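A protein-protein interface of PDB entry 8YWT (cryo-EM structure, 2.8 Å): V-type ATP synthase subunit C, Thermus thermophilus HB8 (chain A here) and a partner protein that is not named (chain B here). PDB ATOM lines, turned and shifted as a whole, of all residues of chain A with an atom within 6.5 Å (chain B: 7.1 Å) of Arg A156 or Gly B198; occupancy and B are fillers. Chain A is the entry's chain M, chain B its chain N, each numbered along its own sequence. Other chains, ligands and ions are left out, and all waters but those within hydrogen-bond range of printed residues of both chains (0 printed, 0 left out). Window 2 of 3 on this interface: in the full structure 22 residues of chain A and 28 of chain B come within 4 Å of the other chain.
Of chain B, only Glu B149, Ala B197 and Gly B198 come within 4 Å of Arg A156.
Gly B198 touches just these residues of chain A: Arg A152 (3.3 Å) and Arg A156 (3.8 Å).
Printed residues of chain B within 4 Å of Arg A152: Glu B149 (2.8 Å) and Gly B198 (3.3 Å).
Of the printed residues of chain A, Ala B200 touches Ala A134 and Gln A138.
Of the printed residues of chain A, Ala B197 touches Arg A156.
Of the printed residues of chain A, Glu B149 touches Arg A152 (2.8 Å) and Arg A156 (2.8 Å).
Leu A155 touches none of the printed residues of chain B.
The nearest residue of chain A that does not touch Gly B198 is Ala A134 (4.1 Å).
The nearest printed residue of chain A that does not touch Ala B197 is Arg A152 (4.5 Å).
Printed residues of chain B that touch a printed residue of chain A: Glu B149, Ala B197, Gly B198 and Ala B200.
Hydrophobic or aromatic side chains of chain B that line the printed part of chain A: Ala B200.
Among the printed residues, Asp or Glu carboxylates within 4 Å of a Lys or Arg side-chain nitrogen of the other chain: Arg A152 with Glu B149 (2.8 Å) and Arg A156 with Glu B149 (2.8 Å).
Ala B200 touches Ala A134 (CB to C, 3.7 Å).
Ala B200 touches Gln A138.
Gly B198 touches Arg A152 (O to CG, 3.3 Å).
N of Gly B198 touches CG of Arg A156, 3.8 Å away.
The side-chain carboxylate of Glu B149 is in salt-bridge range of the guanidinium group of Arg A152.
The guanidinium group (NH1) of Arg A156 lies within salt-bridge range of the side-chain carboxylate (OE1) of Glu B149, at 2.8 Å.
The backbone carbonyl oxygen (O) of Ala B197 is in hydrogen-bond range of the guanidinium group (NH2) of Arg A156 (2.9 Å).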
ATOM      1  N   PRO A 133      23.149  -4.988  -9.024  1.00  0.00           N
ATOM      2  CA  PRO A 133      22.571  -6.257  -9.471  1.00  0.00           C
ATOM      3  C   PRO A 133      21.475  -6.150 -10.543  1.00  0.00           C
ATOM      4  O   PRO A 133      21.412  -6.993 -11.435  1.00  0.00           O
ATOM      5  CB  PRO A 133      22.042  -6.917  -8.200  1.00  0.00           C
ATOM      6  CG  PRO A 133      23.021  -6.428  -7.143  1.00  0.00           C
ATOM      7  CD  PRO A 133      23.262  -4.987  -7.574  1.00  0.00           C
ATOM      8  N   ALA A 134      20.645  -5.107 -10.548  1.00  0.00           N
ATOM      9  CA  ALA A 134      19.689  -4.902 -11.636  1.00  0.00           C
ATOM     10  C   ALA A 134      20.371  -4.478 -12.954  1.00  0.00           C
ATOM     11  O   ALA A 134      19.877  -4.787 -14.035  1.00  0.00           O
ATOM     12  CB  ALA A 134      18.627  -3.904 -11.171  1.00  0.00           C
ATOM     13  N   ALA A 137      21.676  -7.848 -14.314  1.00  0.00           N
ATOM     14  CA  ALA A 137      20.526  -8.478 -14.961  1.00  0.00           C
ATOM     15  C   ALA A 137      20.240  -7.932 -16.370  1.00  0.00           C
ATOM     16  O   ALA A 137      19.854  -8.697 -17.246  1.00  0.00           O
ATOM     17  CB  ALA A 137      19.301  -8.304 -14.065  1.00  0.00           C
ATOM     18  N   GLN A 138      20.463  -6.640 -16.625  1.00  0.00           N
ATOM     19  CA  GLN A 138      20.310  -6.054 -17.961  1.00  0.00           C
ATOM     20  C   GLN A 138      21.388  -6.531 -18.931  1.00  0.00           C
ATOM     21  O   GLN A 138      21.067  -6.861 -20.070  1.00  0.00           O
ATOM     22  CB  GLN A 138      20.323  -4.521 -17.886  1.00  0.00           C
ATOM     23  CG  GLN A 138      19.040  -3.944 -17.284  1.00  0.00           C
ATOM     24  CD  GLN A 138      17.829  -4.161 -18.178  1.00  0.00           C
ATOM     25  OE1 GLN A 138      17.799  -3.758 -19.329  1.00  0.00           O
ATOM     26  NE2 GLN A 138      16.802  -4.827 -17.699  1.00  0.00           N
ATOM     27  N   ARG A 149      16.257 -13.091 -16.535  1.00  0.00           N
ATOM     28  CA  ARG A 149      14.840 -13.202 -16.168  1.00  0.00           C
ATOM     29  C   ARG A 149      14.653 -13.639 -14.714  1.00  0.00           C
ATOM     30  O   ARG A 149      13.851 -13.044 -14.004  1.00  0.00           O
ATOM     31  CB  ARG A 149      14.198 -14.198 -17.141  1.00  0.00           C
ATOM     32  CG  ARG A 149      12.673 -14.269 -17.043  1.00  0.00           C
ATOM     33  CD  ARG A 149      12.114 -15.419 -17.889  1.00  0.00           C
ATOM     34  NE  ARG A 149      12.470 -15.291 -19.316  1.00  0.00           N
ATOM     35  CZ  ARG A 149      11.739 -15.639 -20.359  1.00  0.00           C
ATOM     36  NH1 ARG A 149      12.192 -15.461 -21.563  1.00  0.00           N
ATOM     37  NH2 ARG A 149      10.552 -16.155 -20.242  1.00  0.00           N
ATOM     38  N   LEU A 151      16.988 -13.338 -12.111  1.00  0.00           N
ATOM     39  CA  LEU A 151      17.547 -12.322 -11.213  1.00  0.00           C
ATOM     40  C   LEU A 151      16.615 -11.118 -11.066  1.00  0.00           C
ATOM     41  O   LEU A 151      16.440 -10.637  -9.953  1.00  0.00           O
ATOM     42  CB  LEU A 151      18.947 -11.906 -11.707  1.00  0.00           C
ATOM     43  CG  LEU A 151      19.641 -10.818 -10.864  1.00  0.00           C
ATOM     44  CD1 LEU A 151      19.817 -11.211  -9.400  1.00  0.00           C
ATOM     45  CD2 LEU A 151      21.038 -10.546 -11.414  1.00  0.00           C
ATOM     46  N   ARG A 152      15.938 -10.663 -12.132  1.00  0.00           N
ATOM     47  CA  ARG A 152      14.947  -9.574 -12.015  1.00  0.00           C
ATOM     48  C   ARG A 152      13.791  -9.925 -11.081  1.00  0.00           C
ATOM     49  O   ARG A 152      13.357  -9.078 -10.309  1.00  0.00           O
ATOM     50  CB  ARG A 152      14.417  -9.149 -13.387  1.00  0.00           C
ATOM     51  CG  ARG A 152      15.501  -8.440 -14.201  1.00  0.00           C
ATOM     52  CD  ARG A 152      14.934  -7.683 -15.408  1.00  0.00           C
ATOM     53  NE  ARG A 152      15.231  -8.373 -16.674  1.00  0.00           N
ATOM     54  CZ  ARG A 152      14.448  -9.179 -17.355  1.00  0.00           C
ATOM     55  NH1 ARG A 152      14.892  -9.736 -18.439  1.00  0.00           N
ATOM     56  NH2 ARG A 152      13.229  -9.451 -17.001  1.00  0.00           N
ATOM     57  N   ALA A 153      13.336 -11.173 -11.078  1.00  0.00           N
ATOM     58  CA  ALA A 153      12.337 -11.636 -10.120  1.00  0.00           C
ATOM     59  C   ALA A 153      12.886 -11.662  -8.682  1.00  0.00           C
ATOM     60  O   ALA A 153      12.266 -11.113  -7.775  1.00  0.00           O
ATOM     61  CB  ALA A 153      11.825 -13.005 -10.567  1.00  0.00           C
ATOM     62  N   VAL A 154      14.082 -12.206  -8.466  1.00  0.00           N
ATOM     63  CA  VAL A 154      14.722 -12.182  -7.140  1.00  0.00           C
ATOM     64  C   VAL A 154      14.845 -10.754  -6.597  1.00  0.00           C
ATOM     65  O   VAL A 154      14.517 -10.503  -5.441  1.00  0.00           O
ATOM     66  CB  VAL A 154      16.097 -12.865  -7.186  1.00  0.00           C
ATOM     67  CG1 VAL A 154      16.851 -12.729  -5.871  1.00  0.00           C
ATOM     68  CG2 VAL A 154      15.949 -14.353  -7.486  1.00  0.00           C
ATOM     69  N   LEU A 155      15.253  -9.798  -7.428  1.00  0.00           N
ATOM     70  CA  LEU A 155      15.427  -8.406  -7.020  1.00  0.00           C
ATOM     71  C   LEU A 155      14.108  -7.653  -6.823  1.00  0.00           C
ATOM     72  O   LEU A 155      14.124  -6.566  -6.254  1.00  0.00           O
ATOM     73  CB  LEU A 155      16.330  -7.688  -8.029  1.00  0.00           C
ATOM     74  CG  LEU A 155      17.760  -8.247  -8.112  1.00  0.00           C
ATOM     75  CD1 LEU A 155      18.506  -7.515  -9.218  1.00  0.00           C
ATOM     76  CD2 LEU A 155      18.540  -8.127  -6.808  1.00  0.00           C
ATOM     77  N   ARG A 156      12.956  -8.203  -7.237  1.00  0.00           N
ATOM     78  CA  ARG A 156      11.638  -7.720  -6.783  1.00  0.00           C
ATOM     79  C   ARG A 156      11.302  -8.227  -5.386  1.00  0.00           C
ATOM     80  O   ARG A 156      10.678  -7.499  -4.624  1.00  0.00           O
ATOM     81  CB  ARG A 156      10.527  -8.094  -7.777  1.00  0.00           C
ATOM     82  CG  ARG A 156      10.558  -7.160  -8.994  1.00  0.00           C
ATOM     83  CD  ARG A 156       9.370  -7.372  -9.937  1.00  0.00           C
ATOM     84  NE  ARG A 156       9.491  -8.623 -10.701  1.00  0.00           N
ATOM     85  CZ  ARG A 156      10.051  -8.794 -11.882  1.00  0.00           C
ATOM     86  NH1 ARG A 156      10.021  -9.977 -12.413  1.00  0.00           N
ATOM     87  NH2 ARG A 156      10.632  -7.840 -12.552  1.00  0.00           N
ATOM     88  N   GLU A 157      11.727  -9.431  -5.018  1.00  0.00           N
ATOM     89  CA  GLU A 157      11.501  -9.960  -3.671  1.00  0.00           C
ATOM     90  C   GLU A 157      12.384  -9.302  -2.605  1.00  0.00           C
ATOM     91  O   GLU A 157      11.882  -8.972  -1.531  1.00  0.00           O
ATOM     92  CB  GLU A 157      11.719 -11.476  -3.621  1.00  0.00           C
ATOM     93  CG  GLU A 157      10.757 -12.248  -4.517  1.00  0.00           C
ATOM     94  CD  GLU A 157      10.844 -13.756  -4.252  1.00  0.00           C
ATOM     95  OE1 GLU A 157      10.435 -14.212  -3.159  1.00  0.00           O
ATOM     96  OE2 GLU A 157      11.288 -14.496  -5.156  1.00  0.00           O
ATOM     97  N   THR A 158      13.695  -9.156  -2.826  1.00  0.00           N
ATOM     98  CA  THR A 158      14.655  -8.762  -1.774  1.00  0.00           C
ATOM     99  C   THR A 158      15.948  -8.172  -2.344  1.00  0.00           C
ATOM    100  O   THR A 158      16.373  -8.581  -3.416  1.00  0.00           O
ATOM    101  CB  THR A 158      14.937 -10.004  -0.904  1.00  0.00           C
ATOM    102  OG1 THR A 158      13.831 -10.238  -0.063  1.00  0.00           O
ATOM    103  CG2 THR A 158      16.145  -9.936   0.027  1.00  0.00           C
ATOM    104  N   GLN A 159      16.608  -7.251  -1.622  1.00  0.00           N
ATOM    105  CA  GLN A 159      17.903  -6.650  -2.009  1.00  0.00           C
ATOM    106  C   GLN A 159      19.112  -7.180  -1.208  1.00  0.00           C
ATOM    107  O   GLN A 159      20.257  -6.987  -1.612  1.00  0.00           O
ATOM    108  CB  GLN A 159      17.856  -5.115  -1.866  1.00  0.00           C
ATOM    109  CG  GLN A 159      16.612  -4.401  -2.426  1.00  0.00           C
ATOM    110  CD  GLN A 159      16.254  -4.788  -3.854  1.00  0.00           C
ATOM    111  OE1 GLN A 159      17.098  -5.001  -4.710  1.00  0.00           O
ATOM    112  NE2 GLN A 159      14.985  -4.886  -4.164  1.00  0.00           N
ATOM    113  N   LEU B 145      13.246  -6.143 -21.142  1.00  0.00           N
ATOM    114  CA  LEU B 145      12.268  -6.815 -20.274  1.00  0.00           C
ATOM    115  C   LEU B 145      11.583  -8.006 -20.979  1.00  0.00           C
ATOM    116  O   LEU B 145      11.985  -8.422 -22.061  1.00  0.00           O
ATOM    117  CB  LEU B 145      11.246  -5.754 -19.801  1.00  0.00           C
ATOM    118  CG  LEU B 145      10.722  -6.018 -18.377  1.00  0.00           C
ATOM    119  CD1 LEU B 145      11.727  -5.592 -17.316  1.00  0.00           C
ATOM    120  CD2 LEU B 145       9.422  -5.259 -18.150  1.00  0.00           C
ATOM    121  N   THR B 146      10.528  -8.552 -20.377  1.00  0.00           N
ATOM    122  CA  THR B 146       9.666  -9.618 -20.908  1.00  0.00           C
ATOM    123  C   THR B 146       8.199  -9.289 -20.610  1.00  0.00           C
ATOM    124  O   THR B 146       7.881  -8.662 -19.597  1.00  0.00           O
ATOM    125  CB  THR B 146      10.015 -10.995 -20.315  1.00  0.00           C
ATOM    126  OG1 THR B 146      10.038 -10.948 -18.905  1.00  0.00           O
ATOM    127  CG2 THR B 146      11.364 -11.528 -20.778  1.00  0.00           C
ATOM    128  N   LYS B 148       5.839 -11.022 -19.470  1.00  0.00           N
ATOM    129  CA  LYS B 148       5.450 -11.614 -18.185  1.00  0.00           C
ATOM    130  C   LYS B 148       5.456 -10.600 -17.032  1.00  0.00           C
ATOM    131  O   LYS B 148       4.715 -10.777 -16.069  1.00  0.00           O
ATOM    132  CB  LYS B 148       6.384 -12.807 -17.905  1.00  0.00           C
ATOM    133  CG  LYS B 148       5.898 -13.675 -16.736  1.00  0.00           C
ATOM    134  CD  LYS B 148       6.765 -14.928 -16.567  1.00  0.00           C
ATOM    135  CE  LYS B 148       6.194 -15.903 -15.533  1.00  0.00           C
ATOM    136  NZ  LYS B 148       6.258 -15.384 -14.150  1.00  0.00           N
ATOM    137  N   GLU B 149       6.268  -9.543 -17.116  1.00  0.00           N
ATOM    138  CA  GLU B 149       6.507  -8.618 -15.997  1.00  0.00           C
ATOM    139  C   GLU B 149       6.400  -7.123 -16.333  1.00  0.00           C
ATOM    140  O   GLU B 149       6.505  -6.293 -15.433  1.00  0.00           O
ATOM    141  CB  GLU B 149       7.827  -8.978 -15.299  1.00  0.00           C
ATOM    142  CG  GLU B 149       9.088  -8.674 -16.122  1.00  0.00           C
ATOM    143  CD  GLU B 149      10.340  -9.266 -15.464  1.00  0.00           C
ATOM    144  OE1 GLU B 149      10.336 -10.461 -15.104  1.00  0.00           O
ATOM    145  OE2 GLU B 149      11.314  -8.524 -15.193  1.00  0.00           O
ATOM    146  N   LEU B 150       6.099  -6.751 -17.581  1.00  0.00           N
ATOM    147  CA  LEU B 150       5.854  -5.354 -17.967  1.00  0.00           C
ATOM    148  C   LEU B 150       4.789  -4.621 -17.105  1.00  0.00           C
ATOM    149  O   LEU B 150       5.022  -3.464 -16.745  1.00  0.00           O
ATOM    150  CB  LEU B 150       5.568  -5.327 -19.481  1.00  0.00           C
ATOM    151  CG  LEU B 150       5.352  -3.929 -20.077  1.00  0.00           C
ATOM    152  CD1 LEU B 150       6.581  -3.032 -19.937  1.00  0.00           C
ATOM    153  CD2 LEU B 150       5.050  -4.075 -21.563  1.00  0.00           C
ATOM    154  N   LEU B 152       4.431  -4.877 -13.875  1.00  0.00           N
ATOM    155  CA  LEU B 152       5.111  -4.471 -12.632  1.00  0.00           C
ATOM    156  C   LEU B 152       5.841  -3.138 -12.826  1.00  0.00           C
ATOM    157  O   LEU B 152       5.872  -2.315 -11.913  1.00  0.00           O
ATOM    158  CB  LEU B 152       6.126  -5.534 -12.161  1.00  0.00           C
ATOM    159  CG  LEU B 152       5.582  -6.829 -11.529  1.00  0.00           C
ATOM    160  CD1 LEU B 152       4.770  -6.555 -10.268  1.00  0.00           C
ATOM    161  CD2 LEU B 152       4.741  -7.675 -12.478  1.00  0.00           C
ATOM    162  N   VAL B 153       6.405  -2.911 -14.016  1.00  0.00           N
ATOM    163  CA  VAL B 153       7.050  -1.642 -14.374  1.00  0.00           C
ATOM    164  C   VAL B 153       6.014  -0.534 -14.536  1.00  0.00           C
ATOM    165  O   VAL B 153       6.194   0.546 -13.980  1.00  0.00           O
ATOM    166  CB  VAL B 153       7.923  -1.800 -15.630  1.00  0.00           C
ATOM    167  CG1 VAL B 153       8.480  -0.457 -16.106  1.00  0.00           C
ATOM    168  CG2 VAL B 153       9.109  -2.725 -15.336  1.00  0.00           C
ATOM    169  N   ALA B 192      14.493   5.067  -9.526  1.00  0.00           N
ATOM    170  CA  ALA B 192      14.024   4.421  -8.296  1.00  0.00           C
ATOM    171  C   ALA B 192      12.810   3.498  -8.535  1.00  0.00           C
ATOM    172  O   ALA B 192      12.779   2.377  -8.034  1.00  0.00           O
ATOM    173  CB  ALA B 192      13.712   5.506  -7.263  1.00  0.00           C
ATOM    174  N   ALA B 193      11.833   3.921  -9.342  1.00  0.00           N
ATOM    175  CA  ALA B 193      10.667   3.112  -9.698  1.00  0.00           C
ATOM    176  C   ALA B 193      11.075   1.815 -10.414  1.00  0.00           C
ATOM    177  O   ALA B 193      10.697   0.724  -9.994  1.00  0.00           O
ATOM    178  CB  ALA B 193       9.731   3.956 -10.569  1.00  0.00           C
ATOM    179  N   LEU B 194      11.918   1.920 -11.441  1.00  0.00           N
ATOM    180  CA  LEU B 194      12.469   0.769 -12.148  1.00  0.00           C
ATOM    181  C   LEU B 194      13.230  -0.150 -11.182  1.00  0.00           C
ATOM    182  O   LEU B 194      12.969  -1.350 -11.162  1.00  0.00           O
ATOM    183  CB  LEU B 194      13.362   1.268 -13.299  1.00  0.00           C
ATOM    184  CG  LEU B 194      12.596   1.976 -14.433  1.00  0.00           C
ATOM    185  CD1 LEU B 194      13.588   2.663 -15.366  1.00  0.00           C
ATOM    186  CD2 LEU B 194      11.759   1.005 -15.260  1.00  0.00           C
ATOM    187  N   SER B 195      14.077   0.402 -10.308  1.00  0.00           N
ATOM    188  CA  SER B 195      14.800  -0.378  -9.290  1.00  0.00           C
ATOM    189  C   SER B 195      13.857  -1.190  -8.394  1.00  0.00           C
ATOM    190  O   SER B 195      14.089  -2.379  -8.172  1.00  0.00           O
ATOM    191  CB  SER B 195      15.675   0.561  -8.457  1.00  0.00           C
ATOM    192  OG  SER B 195      16.359  -0.134  -7.437  1.00  0.00           O
ATOM    193  N   ARG B 196      12.729  -0.616  -7.956  1.00  0.00           N
ATOM    194  CA  ARG B 196      11.691  -1.322  -7.176  1.00  0.00           C
ATOM    195  C   ARG B 196      10.932  -2.382  -7.984  1.00  0.00           C
ATOM    196  O   ARG B 196      10.403  -3.322  -7.401  1.00  0.00           O
ATOM    197  CB  ARG B 196      10.721  -0.299  -6.563  1.00  0.00           C
ATOM    198  CG  ARG B 196      11.414   0.547  -5.486  1.00  0.00           C
ATOM    199  CD  ARG B 196      10.532   1.708  -5.032  1.00  0.00           C
ATOM    200  NE  ARG B 196      11.262   2.570  -4.085  1.00  0.00           N
ATOM    201  CZ  ARG B 196      11.226   3.887  -4.000  1.00  0.00           C
ATOM    202  NH1 ARG B 196      11.975   4.506  -3.142  1.00  0.00           N
ATOM    203  NH2 ARG B 196      10.457   4.617  -4.753  1.00  0.00           N
ATOM    204  N   ALA B 197      10.911  -2.283  -9.314  1.00  0.00           N
ATOM    205  CA  ALA B 197      10.446  -3.334 -10.224  1.00  0.00           C
ATOM    206  C   ALA B 197      11.535  -4.371 -10.586  1.00  0.00           C
ATOM    207  O   ALA B 197      11.270  -5.277 -11.376  1.00  0.00           O
ATOM    208  CB  ALA B 197       9.856  -2.677 -11.480  1.00  0.00           C
ATOM    209  N   GLY B 198      12.753  -4.267 -10.035  1.00  0.00           N
ATOM    210  CA  GLY B 198      13.882  -5.141 -10.372  1.00  0.00           C
ATOM    211  C   GLY B 198      14.540  -4.815 -11.717  1.00  0.00           C
ATOM    212  O   GLY B 198      15.134  -5.696 -12.329  1.00  0.00           O
ATOM    213  N   VAL B 199      14.418  -3.575 -12.194  1.00  0.00           N
ATOM    214  CA  VAL B 199      14.865  -3.091 -13.511  1.00  0.00           C
ATOM    215  C   VAL B 199      15.869  -1.942 -13.352  1.00  0.00           C
ATOM    216  O   VAL B 199      15.839  -1.204 -12.373  1.00  0.00           O
ATOM    217  CB  VAL B 199      13.650  -2.671 -14.364  1.00  0.00           C
ATOM    218  CG1 VAL B 199      14.014  -2.154 -15.758  1.00  0.00           C
ATOM    219  CG2 VAL B 199      12.697  -3.852 -14.568  1.00  0.00           C
ATOM    220  N   ALA B 200      16.772  -1.778 -14.314  1.00  0.00           N
ATOM    221  CA  ALA B 200      17.713  -0.665 -14.401  1.00  0.00           C
ATOM    222  C   ALA B 200      17.920  -0.242 -15.865  1.00  0.00           C
ATOM    223  O   ALA B 200      17.510  -0.944 -16.786  1.00  0.00           O
ATOM    224  CB  ALA B 200      19.023  -1.079 -13.731  1.00  0.00           C
